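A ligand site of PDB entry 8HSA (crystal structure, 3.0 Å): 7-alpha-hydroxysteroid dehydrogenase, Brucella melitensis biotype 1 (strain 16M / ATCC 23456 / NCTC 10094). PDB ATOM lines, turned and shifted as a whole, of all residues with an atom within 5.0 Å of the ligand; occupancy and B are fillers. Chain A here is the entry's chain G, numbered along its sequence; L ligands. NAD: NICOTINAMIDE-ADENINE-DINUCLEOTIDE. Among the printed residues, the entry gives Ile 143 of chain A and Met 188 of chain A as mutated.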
ATOM      1  N   THR A  13       2.439 -10.661  16.679  1.00  0.00           N
ATOM      2  CA  THR A  13       3.238 -10.399  15.488  1.00  0.00           C
ATOM      3  C   THR A  13       2.341 -10.248  14.266  1.00  0.00           C
ATOM      4  O   THR A  13       1.403 -11.020  14.063  1.00  0.00           O
ATOM      5  CB  THR A  13       4.261 -11.513  15.230  1.00  0.00           C
ATOM      6  OG1 THR A  13       3.605 -12.707  14.784  1.00  0.00           O
ATOM      7  CG2 THR A  13       5.045 -11.796  16.510  1.00  0.00           C
ATOM      8  N   GLY A  14       2.621  -9.234  13.452  1.00  0.00           N
ATOM      9  CA  GLY A  14       1.879  -9.041  12.228  1.00  0.00           C
ATOM     10  C   GLY A  14       0.619  -8.243  12.395  1.00  0.00           C
ATOM     11  O   GLY A  14      -0.337  -8.449  11.647  1.00  0.00           O
ATOM     12  N   ALA A  15       0.600  -7.306  13.326  1.00  0.00           N
ATOM     13  CA  ALA A  15      -0.637  -6.692  13.798  1.00  0.00           C
ATOM     14  C   ALA A  15      -0.835  -5.258  13.317  1.00  0.00           C
ATOM     15  O   ALA A  15      -1.322  -4.421  14.078  1.00  0.00           O
ATOM     16  CB  ALA A  15      -0.683  -6.726  15.319  1.00  0.00           C
ATOM     17  N   ALA A  16      -0.500  -4.944  12.053  1.00  0.00           N
ATOM     18  CA  ALA A  16      -0.663  -3.569  11.592  1.00  0.00           C
ATOM     19  C   ALA A  16      -2.044  -3.302  10.971  1.00  0.00           C
ATOM     20  O   ALA A  16      -2.623  -2.230  11.208  1.00  0.00           O
ATOM     21  CB  ALA A  16       0.425  -3.192  10.589  1.00  0.00           C
ATOM     22  N   ALA A  17      -2.581  -4.229  10.175  1.00  0.00           N
ATOM     23  CA  ALA A  17      -3.996  -4.237   9.840  1.00  0.00           C
ATOM     24  C   ALA A  17      -4.477  -5.683   9.858  1.00  0.00           C
ATOM     25  O   ALA A  17      -3.700  -6.613  10.129  1.00  0.00           O
ATOM     26  CB  ALA A  17      -4.285  -3.554   8.498  1.00  0.00           C
ATOM     27  N   GLY A  18      -5.774  -5.856   9.588  1.00  0.00           N
ATOM     28  CA  GLY A  18      -6.451  -7.136   9.565  1.00  0.00           C
ATOM     29  C   GLY A  18      -6.603  -7.836  10.901  1.00  0.00           C
ATOM     30  O   GLY A  18      -6.928  -7.220  11.922  1.00  0.00           O
ATOM     31  N   ILE A  19      -6.350  -9.143  10.890  1.00  0.00           N
ATOM     32  CA  ILE A  19      -6.521  -9.957  12.099  1.00  0.00           C
ATOM     33  C   ILE A  19      -5.556  -9.531  13.189  1.00  0.00           C
ATOM     34  O   ILE A  19      -5.957  -9.330  14.346  1.00  0.00           O
ATOM     35  CB  ILE A  19      -6.351 -11.458  11.781  1.00  0.00           C
ATOM     36  CG1 ILE A  19      -7.581 -12.004  11.048  1.00  0.00           C
ATOM     37  CG2 ILE A  19      -6.122 -12.222  13.021  1.00  0.00           C
ATOM     38  CD1 ILE A  19      -7.344 -13.341  10.365  1.00  0.00           C
ATOM     39  N   GLY A  20      -4.258  -9.428  12.862  1.00  0.00           N
ATOM     40  CA  GLY A  20      -3.279  -8.934  13.802  1.00  0.00           C
ATOM     41  C   GLY A  20      -3.714  -7.657  14.469  1.00  0.00           C
ATOM     42  O   GLY A  20      -3.840  -7.609  15.701  1.00  0.00           O
ATOM     43  N   ASP A  38       5.052  -5.490  13.763  1.00  0.00           N
ATOM     44  CA  ASP A  38       4.781  -5.832  12.378  1.00  0.00           C
ATOM     45  C   ASP A  38       6.074  -5.645  11.604  1.00  0.00           C
ATOM     46  O   ASP A  38       7.078  -5.168  12.146  1.00  0.00           O
ATOM     47  CB  ASP A  38       3.663  -4.947  11.837  1.00  0.00           C
ATOM     48  CG  ASP A  38       3.034  -5.502  10.599  1.00  0.00           C
ATOM     49  OD1 ASP A  38       3.772  -5.677   9.610  1.00  0.00           O
ATOM     50  OD2 ASP A  38       1.812  -5.777  10.625  1.00  0.00           O
ATOM     51  N   LEU A  39       6.061  -6.042  10.327  1.00  0.00           N
ATOM     52  CA  LEU A  39       7.216  -5.727   9.492  1.00  0.00           C
ATOM     53  C   LEU A  39       7.227  -4.251   9.102  1.00  0.00           C
ATOM     54  O   LEU A  39       8.300  -3.664   8.908  1.00  0.00           O
ATOM     55  CB  LEU A  39       7.253  -6.602   8.237  1.00  0.00           C
ATOM     56  CG  LEU A  39       8.631  -6.791   7.566  1.00  0.00           C
ATOM     57  CD1 LEU A  39       8.624  -8.029   6.702  1.00  0.00           C
ATOM     58  CD2 LEU A  39       9.160  -5.597   6.741  1.00  0.00           C
ATOM     59  N   LYS A  40       6.048  -3.644   8.979  1.00  0.00           N
ATOM     60  CA  LYS A  40       5.905  -2.239   8.604  1.00  0.00           C
ATOM     61  C   LYS A  40       5.714  -1.431   9.884  1.00  0.00           C
ATOM     62  O   LYS A  40       4.589  -1.223  10.353  1.00  0.00           O
ATOM     63  CB  LYS A  40       4.773  -2.049   7.604  1.00  0.00           C
ATOM     64  CG  LYS A  40       4.893  -2.930   6.339  1.00  0.00           C
ATOM     65  CD  LYS A  40       6.152  -2.626   5.498  1.00  0.00           C
ATOM     66  CE  LYS A  40       6.208  -3.485   4.216  1.00  0.00           C
ATOM     67  NZ  LYS A  40       7.448  -3.284   3.409  1.00  0.00           N
ATOM     68  N   CYS A  63       9.195  -5.876  13.342  1.00  0.00           N
ATOM     69  CA  CYS A  63       9.674  -7.258  13.477  1.00  0.00           C
ATOM     70  C   CYS A  63       9.216  -8.093  12.284  1.00  0.00           C
ATOM     71  O   CYS A  63       8.064  -8.541  12.242  1.00  0.00           O
ATOM     72  CB  CYS A  63       9.202  -7.894  14.761  1.00  0.00           C
ATOM     73  SG  CYS A  63       9.774  -9.577  14.888  1.00  0.00           S
ATOM     74  N   ASN A  64      10.137  -8.319  11.360  1.00  0.00           N
ATOM     75  CA  ASN A  64      10.017  -9.370  10.378  1.00  0.00           C
ATOM     76  C   ASN A  64      10.268 -10.672  11.102  1.00  0.00           C
ATOM     77  O   ASN A  64      11.416 -11.054  11.309  1.00  0.00           O
ATOM     78  CB  ASN A  64      11.035  -9.190   9.258  1.00  0.00           C
ATOM     79  CG  ASN A  64      10.910 -10.231   8.161  1.00  0.00           C
ATOM     80  OD1 ASN A  64      10.035 -11.111   8.200  1.00  0.00           O
ATOM     81  ND2 ASN A  64      11.819 -10.168   7.193  1.00  0.00           N
ATOM     82  N   VAL A  65       9.188 -11.362  11.475  1.00  0.00           N
ATOM     83  CA  VAL A  65       9.305 -12.600  12.256  1.00  0.00           C
ATOM     84  C   VAL A  65      10.346 -13.531  11.641  1.00  0.00           C
ATOM     85  O   VAL A  65      10.995 -14.307  12.347  1.00  0.00           O
ATOM     86  CB  VAL A  65       7.941 -13.276  12.350  1.00  0.00           C
ATOM     87  CG1 VAL A  65       6.985 -12.403  13.155  1.00  0.00           C
ATOM     88  CG2 VAL A  65       7.420 -13.522  10.961  1.00  0.00           C
ATOM     89  N   THR A  66      10.539 -13.440  10.331  1.00  0.00           N
ATOM     90  CA  THR A  66      11.552 -14.244   9.677  1.00  0.00           C
ATOM     91  C   THR A  66      12.968 -13.801  10.058  1.00  0.00           C
ATOM     92  O   THR A  66      13.933 -14.547   9.803  1.00  0.00           O
ATOM     93  CB  THR A  66      11.305 -14.207   8.168  1.00  0.00           C
ATOM     94  OG1 THR A  66      11.707 -12.944   7.630  1.00  0.00           O
ATOM     95  CG2 THR A  66       9.806 -14.357   7.889  1.00  0.00           C
ATOM     96  N   ASN A  91       0.453 -14.271  14.779  1.00  0.00           N
ATOM     97  CA  ASN A  91      -0.491 -14.074  13.686  1.00  0.00           C
ATOM     98  C   ASN A  91       0.168 -13.774  12.353  1.00  0.00           C
ATOM     99  O   ASN A  91      -0.396 -14.129  11.318  1.00  0.00           O
ATOM    100  CB  ASN A  91      -1.478 -12.964  14.017  1.00  0.00           C
ATOM    101  CG  ASN A  91      -2.164 -12.416  12.792  1.00  0.00           C
ATOM    102  OD1 ASN A  91      -1.970 -11.255  12.454  1.00  0.00           O
ATOM    103  ND2 ASN A  91      -2.940 -13.239  12.100  1.00  0.00           N
ATOM    104  N   ALA A  92       1.335 -13.144  12.358  1.00  0.00           N
ATOM    105  CA  ALA A  92       2.104 -12.910  11.133  1.00  0.00           C
ATOM    106  C   ALA A  92       2.326 -14.189  10.334  1.00  0.00           C
ATOM    107  O   ALA A  92       2.610 -15.243  10.895  1.00  0.00           O
ATOM    108  CB  ALA A  92       3.452 -12.281  11.478  1.00  0.00           C
ATOM    109  N   GLY A  93       2.198 -14.081   9.026  1.00  0.00           N
ATOM    110  CA  GLY A  93       2.245 -15.228   8.149  1.00  0.00           C
ATOM    111  C   GLY A  93       1.461 -14.923   6.891  1.00  0.00           C
ATOM    112  O   GLY A  93       1.129 -13.771   6.611  1.00  0.00           O
ATOM    113  N   GLY A  94       1.166 -15.955   6.124  1.00  0.00           N
ATOM    114  CA  GLY A  94       0.279 -15.772   4.988  1.00  0.00           C
ATOM    115  C   GLY A  94       0.350 -16.965   4.046  1.00  0.00           C
ATOM    116  O   GLY A  94       0.781 -18.053   4.418  1.00  0.00           O
ATOM    117  N   LEU A 113       7.947 -18.385   6.721  1.00  0.00           N
ATOM    118  CA  LEU A 113       7.036 -17.369   7.201  1.00  0.00           C
ATOM    119  C   LEU A 113       6.012 -17.980   8.150  1.00  0.00           C
ATOM    120  O   LEU A 113       5.868 -17.527   9.286  1.00  0.00           O
ATOM    121  CB  LEU A 113       6.366 -16.646   6.031  1.00  0.00           C
ATOM    122  CG  LEU A 113       5.306 -15.577   6.318  1.00  0.00           C
ATOM    123  CD1 LEU A 113       5.815 -14.459   7.201  1.00  0.00           C
ATOM    124  CD2 LEU A 113       4.741 -14.995   5.047  1.00  0.00           C
ATOM    125  N   ASN A 114       5.355 -19.065   7.722  1.00  0.00           N
ATOM    126  CA  ASN A 114       4.173 -19.610   8.393  1.00  0.00           C
ATOM    127  C   ASN A 114       4.485 -20.579   9.525  1.00  0.00           C
ATOM    128  O   ASN A 114       3.621 -20.784  10.375  1.00  0.00           O
ATOM    129  CB  ASN A 114       3.276 -20.350   7.408  1.00  0.00           C
ATOM    130  CG  ASN A 114       2.554 -19.417   6.458  1.00  0.00           C
ATOM    131  OD1 ASN A 114       2.379 -18.227   6.728  1.00  0.00           O
ATOM    132  ND2 ASN A 114       2.114 -19.964   5.324  1.00  0.00           N
ATOM    133  N   ILE A 140      -2.003 -18.550  14.488  1.00  0.00           N
ATOM    134  CA  ILE A 140      -3.121 -18.301  13.584  1.00  0.00           C
ATOM    135  C   ILE A 140      -2.916 -19.155  12.338  1.00  0.00           C
ATOM    136  O   ILE A 140      -2.108 -18.837  11.475  1.00  0.00           O
ATOM    137  CB  ILE A 140      -3.275 -16.805  13.256  1.00  0.00           C
ATOM    138  CG1 ILE A 140      -3.367 -15.972  14.534  1.00  0.00           C
ATOM    139  CG2 ILE A 140      -4.485 -16.559  12.387  1.00  0.00           C
ATOM    140  CD1 ILE A 140      -4.709 -16.057  15.246  1.00  0.00           C
ATOM    141  N   SER A 141      -3.624 -20.272  12.281  1.00  0.00           N
ATOM    142  CA  SER A 141      -3.385 -21.204  11.196  1.00  0.00           C
ATOM    143  C   SER A 141      -4.235 -20.826   9.986  1.00  0.00           C
ATOM    144  O   SER A 141      -4.168 -19.689   9.524  1.00  0.00           O
ATOM    145  CB  SER A 141      -3.668 -22.630  11.644  1.00  0.00           C
ATOM    146  OG  SER A 141      -3.250 -23.523  10.647  1.00  0.00           O
ATOM    147  N   SER A 142      -5.041 -21.752   9.481  1.00  0.00           N
ATOM    148  CA  SER A 142      -5.881 -21.530   8.310  1.00  0.00           C
ATOM    149  C   SER A 142      -6.787 -22.721   8.067  1.00  0.00           C
ATOM    150  O   SER A 142      -6.517 -23.829   8.542  1.00  0.00           O
ATOM    151  CB  SER A 142      -5.053 -21.292   7.056  1.00  0.00           C
ATOM    152  OG  SER A 142      -5.930 -21.177   5.951  1.00  0.00           O
ATOM    153  N   ILE A 143      -7.852 -22.509   7.274  1.00  0.00           N
ATOM    154  CA  ILE A 143      -8.673 -23.641   6.882  1.00  0.00           C
ATOM    155  C   ILE A 143      -7.932 -24.501   5.872  1.00  0.00           C
ATOM    156  O   ILE A 143      -8.284 -25.675   5.692  1.00  0.00           O
ATOM    157  CB  ILE A 143     -10.064 -23.263   6.332  1.00  0.00           C
ATOM    158  CG1 ILE A 143      -9.981 -22.646   4.937  1.00  0.00           C
ATOM    159  CG2 ILE A 143     -10.817 -22.389   7.312  1.00  0.00           C
ATOM    160  CD1 ILE A 143     -11.369 -22.406   4.273  1.00  0.00           C
ATOM    161  N   TYR A 155       0.798 -23.622   0.651  1.00  0.00           N
ATOM    162  CA  TYR A 155      -0.073 -23.000   1.644  1.00  0.00           C
ATOM    163  C   TYR A 155      -0.785 -24.028   2.518  1.00  0.00           C
ATOM    164  O   TYR A 155      -0.921 -23.848   3.734  1.00  0.00           O
ATOM    165  CB  TYR A 155      -1.065 -22.077   0.934  1.00  0.00           C
ATOM    166  CG  TYR A 155      -1.985 -21.357   1.856  1.00  0.00           C
ATOM    167  CD1 TYR A 155      -1.497 -20.564   2.862  1.00  0.00           C
ATOM    168  CD2 TYR A 155      -3.351 -21.361   1.646  1.00  0.00           C
ATOM    169  CE1 TYR A 155      -2.326 -19.880   3.710  1.00  0.00           C
ATOM    170  CE2 TYR A 155      -4.190 -20.650   2.471  1.00  0.00           C
ATOM    171  CZ  TYR A 155      -3.668 -19.912   3.505  1.00  0.00           C
ATOM    172  OH  TYR A 155      -4.477 -19.191   4.349  1.00  0.00           O
ATOM    173  N   LYS A 159       0.591 -24.806   6.719  1.00  0.00           N
ATOM    174  CA  LYS A 159      -0.292 -24.494   7.796  1.00  0.00           C
ATOM    175  C   LYS A 159      -0.781 -25.739   8.527  1.00  0.00           C
ATOM    176  O   LYS A 159      -1.310 -25.622   9.608  1.00  0.00           O
ATOM    177  CB  LYS A 159      -1.415 -23.623   7.217  1.00  0.00           C
ATOM    178  CG  LYS A 159      -0.926 -22.437   6.425  1.00  0.00           C
ATOM    179  CD  LYS A 159      -1.533 -21.161   6.964  1.00  0.00           C
ATOM    180  CE  LYS A 159      -0.890 -20.760   8.274  1.00  0.00           C
ATOM    181  NZ  LYS A 159      -0.402 -19.364   8.224  1.00  0.00           N
ATOM    182  N   PRO A 185      -8.638 -19.588  10.479  1.00  0.00           N
ATOM    183  CA  PRO A 185      -9.702 -18.758   9.925  1.00  0.00           C
ATOM    184  C   PRO A 185     -10.066 -19.179   8.500  1.00  0.00           C
ATOM    185  O   PRO A 185      -9.268 -19.789   7.780  1.00  0.00           O
ATOM    186  CB  PRO A 185      -9.111 -17.355   9.939  1.00  0.00           C
ATOM    187  CG  PRO A 185      -7.863 -17.464  10.760  1.00  0.00           C
ATOM    188  CD  PRO A 185      -7.382 -18.842  10.530  1.00  0.00           C
ATOM    189  N   GLY A 186     -11.288 -18.828   8.112  1.00  0.00           N
ATOM    190  CA  GLY A 186     -11.724 -18.918   6.728  1.00  0.00           C
ATOM    191  C   GLY A 186     -11.310 -17.681   5.949  1.00  0.00           C
ATOM    192  O   GLY A 186     -10.274 -17.067   6.223  1.00  0.00           O
ATOM    193  N   ALA A 187     -12.133 -17.289   4.979  1.00  0.00           N
ATOM    194  CA  ALA A 187     -11.890 -16.047   4.278  1.00  0.00           C
ATOM    195  C   ALA A 187     -12.400 -14.851   5.073  1.00  0.00           C
ATOM    196  O   ALA A 187     -13.471 -14.897   5.674  1.00  0.00           O
ATOM    197  CB  ALA A 187     -12.577 -16.078   2.908  1.00  0.00           C
ATOM    198  N   MET A 188     -11.618 -13.758   5.049  1.00  0.00           N
ATOM    199  CA  MET A 188     -11.929 -12.545   5.813  1.00  0.00           C
ATOM    200  C   MET A 188     -11.963 -11.307   4.930  1.00  0.00           C
ATOM    201  O   MET A 188     -11.032 -11.056   4.156  1.00  0.00           O
ATOM    202  CB  MET A 188     -10.915 -12.304   6.925  1.00  0.00           C
ATOM    203  CG  MET A 188     -10.249 -13.552   7.405  1.00  0.00           C
ATOM    204  SD  MET A 188     -11.445 -14.197   8.551  1.00  0.00           S
ATOM    205  CE  MET A 188     -11.637 -12.745   9.594  1.00  0.00           C
ATOM    206  N   THR A 190     -10.751  -8.373   4.584  1.00  0.00           N
ATOM    207  CA  THR A 190      -9.561  -7.673   5.066  1.00  0.00           C
ATOM    208  C   THR A 190      -8.869  -6.839   3.981  1.00  0.00           C
ATOM    209  O   THR A 190      -7.640  -6.803   3.875  1.00  0.00           O
ATOM    210  CB  THR A 190      -8.535  -8.665   5.635  1.00  0.00           C
ATOM    211  OG1 THR A 190      -8.221  -9.647   4.646  1.00  0.00           O
ATOM    212  CG2 THR A 190      -9.053  -9.341   6.899  1.00  0.00           C
HETATM  213  PA  NAD L   1      -1.947 -10.396   5.719  1.00  0.00           P
HETATM  214  O1A NAD L   1      -0.861 -11.152   5.018  1.00  0.00           O
HETATM  215  O2A NAD L   1      -3.090  -9.808   4.934  1.00  0.00           O
HETATM  216  O5B NAD L   1      -1.268  -9.193   6.526  1.00  0.00           O
HETATM  217  C5B NAD L   1      -1.776  -8.800   7.794  1.00  0.00           C
HETATM  218  C4B NAD L   1      -0.669  -8.134   8.593  1.00  0.00           C
HETATM  219  O4B NAD L   1       0.467  -9.005   8.699  1.00  0.00           O
HETATM  220  C3B NAD L   1      -0.184  -6.868   7.907  1.00  0.00           C
HETATM  221  O3B NAD L   1      -0.314  -5.760   8.793  1.00  0.00           O
HETATM  222  C2B NAD L   1       1.255  -7.119   7.590  1.00  0.00           C
HETATM  223  O2B NAD L   1       2.028  -5.946   7.748  1.00  0.00           O
HETATM  224  C1B NAD L   1       1.645  -8.207   8.574  1.00  0.00           C
HETATM  225  N9A NAD L   1       2.818  -8.974   8.098  1.00  0.00           N
HETATM  226  C8A NAD L   1       2.976  -9.529   6.888  1.00  0.00           C
HETATM  227  N7A NAD L   1       4.177 -10.142   6.797  1.00  0.00           N
HETATM  228  C5A NAD L   1       4.809  -9.975   7.968  1.00  0.00           C
HETATM  229  C6A NAD L   1       6.110 -10.360   8.545  1.00  0.00           C
HETATM  230  N6A NAD L   1       7.008 -11.073   7.838  1.00  0.00           N
HETATM  231  N1A NAD L   1       6.374  -9.980   9.802  1.00  0.00           N
HETATM  232  C2A NAD L   1       5.501  -9.278  10.527  1.00  0.00           C
HETATM  233  N3A NAD L   1       4.303  -8.886  10.068  1.00  0.00           N
HETATM  234  C4A NAD L   1       3.906  -9.203   8.813  1.00  0.00           C
HETATM  235  O3  NAD L   1      -2.523 -11.307   6.918  1.00  0.00           O
HETATM  236  PN  NAD L   1      -4.068 -11.521   7.313  1.00  0.00           P
HETATM  237  O1N NAD L   1      -4.913 -11.585   6.072  1.00  0.00           O
HETATM  238  O2N NAD L   1      -4.471 -10.595   8.428  1.00  0.00           O
HETATM  239  O5D NAD L   1      -3.904 -12.985   7.936  1.00  0.00           O
HETATM  240  C5D NAD L   1      -2.630 -13.352   8.458  1.00  0.00           C
HETATM  241  C4D NAD L   1      -2.662 -14.759   9.024  1.00  0.00           C
HETATM  242  O4D NAD L   1      -3.989 -15.283   8.997  1.00  0.00           O
HETATM  243  C3D NAD L   1      -1.803 -15.683   8.187  1.00  0.00           C
HETATM  244  O3D NAD L   1      -0.978 -16.477   9.031  1.00  0.00           O
HETATM  245  C2D NAD L   1      -2.758 -16.566   7.437  1.00  0.00           C
HETATM  246  O2D NAD L   1      -2.243 -17.897   7.343  1.00  0.00           O
HETATM  247  C1D NAD L   1      -4.031 -16.510   8.268  1.00  0.00           C
HETATM  248  N1N NAD L   1      -5.207 -16.544   7.398  1.00  0.00           N
HETATM  249  C2N NAD L   1      -5.773 -15.420   6.962  1.00  0.00           C
HETATM  250  C3N NAD L   1      -6.885 -15.499   6.141  1.00  0.00           C
HETATM  251  C7N NAD L   1      -7.546 -14.254   5.629  1.00  0.00           C
HETATM  252  O7N NAD L   1      -8.389 -14.341   4.763  1.00  0.00           O
HETATM  253  N7N NAD L   1      -7.200 -13.085   6.142  1.00  0.00           N
HETATM  254  C4N NAD L   1      -7.399 -16.719   5.788  1.00  0.00           C
HETATM  255  C5N NAD L   1      -6.792 -17.863   6.259  1.00  0.00           C
HETATM  256  C6N NAD L   1      -5.687 -17.732   7.067  1.00  0.00           C
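The backbone carbonyl oxygen (O) of Ser 141 is in hydrogen-bond range of an oxygen (O2D) of the ligand (3.4 Å).
N3A of the ligand sits close to N of Leu 39, at 3.4 Å.
The backbone NH (N) of Met 188 sits at hydrogen-bond distance from an oxygen (O7N) of the ligand, at 3.3 Å.
N of Ala 16 lies close to O3B of the ligand, 3.4 Å away.
OD1 of Asn 64 lies within hydrogen-bond range of N6A of the ligand.
O2B of the ligand sits at hydrogen-bond distance from OD1 of Asp 38, 2.6 Å away.
NZ of Lys 159 sits at hydrogen-bond distance from O2D of the ligand, at 2.5 Å.
N of Ala 17 lies within hydrogen-bond range of O3B of the ligand (3.1 Å).
O of Asn 91 lies close to O3D of the ligand, 3.3 Å away.
N of Ile 19 is in hydrogen-bond range of O2N of the ligand (3.4 Å).
NZ of Lys 159 lies within hydrogen-bond range of OD1 of Asn 114, 3.4 Å away.
The backbone carbonyl oxygen of Gly 14 sits close to the side-chain amide oxygen of Asn 91 (3.3 Å).
The side-chain hydroxyl (OG) of Ser 142 lies within hydrogen-bond range of the side-chain hydroxyl (OH) of Tyr 155, 2.9 Å away.
The side-chain carboxylate (OD2) of Asp 38 is in hydrogen-bond range of the backbone NH (N) of Ala 16 (2.8 Å).
The backbone carbonyl oxygen of Thr 13 lies within hydrogen-bond range of the backbone NH of Asn 91 (3.5 Å).
The backbone carbonyl oxygen (O) of Thr 13 lies within hydrogen-bond range of the backbone NH (N) of Ala 92.
The side-chain carboxylate (OD1) of Asp 38 is in hydrogen-bond range of the backbone NH (N) of Lys 40 (3.1 Å).
The backbone carbonyl oxygen (O) of Lys 159 sits at hydrogen-bond distance from the side-chain hydroxyl (OG) of Ser 141, at 3.0 Å.
An oxygen (O4B) of the ligand lies close to the backbone carbonyl oxygen (O) of Gly 14 (3.1 Å).
The backbone carbonyl oxygen (O) of Cys 63 lies close to a nitrogen (N1A) of the ligand, 3.3 Å away.
Val 65 touches the ligand.
CB of Ala 92 touches C2A of the ligand, at 3.8 Å.
CA of Gly 93 touches O3D of the ligand (3.6 Å).
Gly 94 touches the ligand (N to C3D, 3.6 Å).
Leu 113 touches the ligand (CD1 to N6A, 3.6 Å).
Ile 140 touches the ligand (O to O3D, 3.6 Å).
OG of Ser 142 touches C5N of the ligand, 3.4 Å away.
Tyr 155 touches the ligand.
O of Pro 185 touches C5N of the ligand, at 3.5 Å.
Gly 186 touches the ligand (O to C4N, 2.9 Å).
Ala 187 touches the ligand (CA to O7N, 3.9 Å).
Thr 190 touches the ligand.
Hydrophobic or aromatic side chains that line the ligand: Ala 16, Ile 19, Leu 39, Val 65, Ala 92, Leu 113, Ile 140 and Met 188.
Within 4 Å of the ligand: Gly 14, Ala 16, Ala 17, Ile 19, Asp 38, Leu 39, Cys 63, Asn 64, Val 65, Asn 91, Ala 92, Gly 93, Gly 94, Leu 113, Ile 140, Ser 141, Ser 142, Tyr 155, Lys 159, Pro 185, Gly 186, Ala 187, Met 188 and Thr 190.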
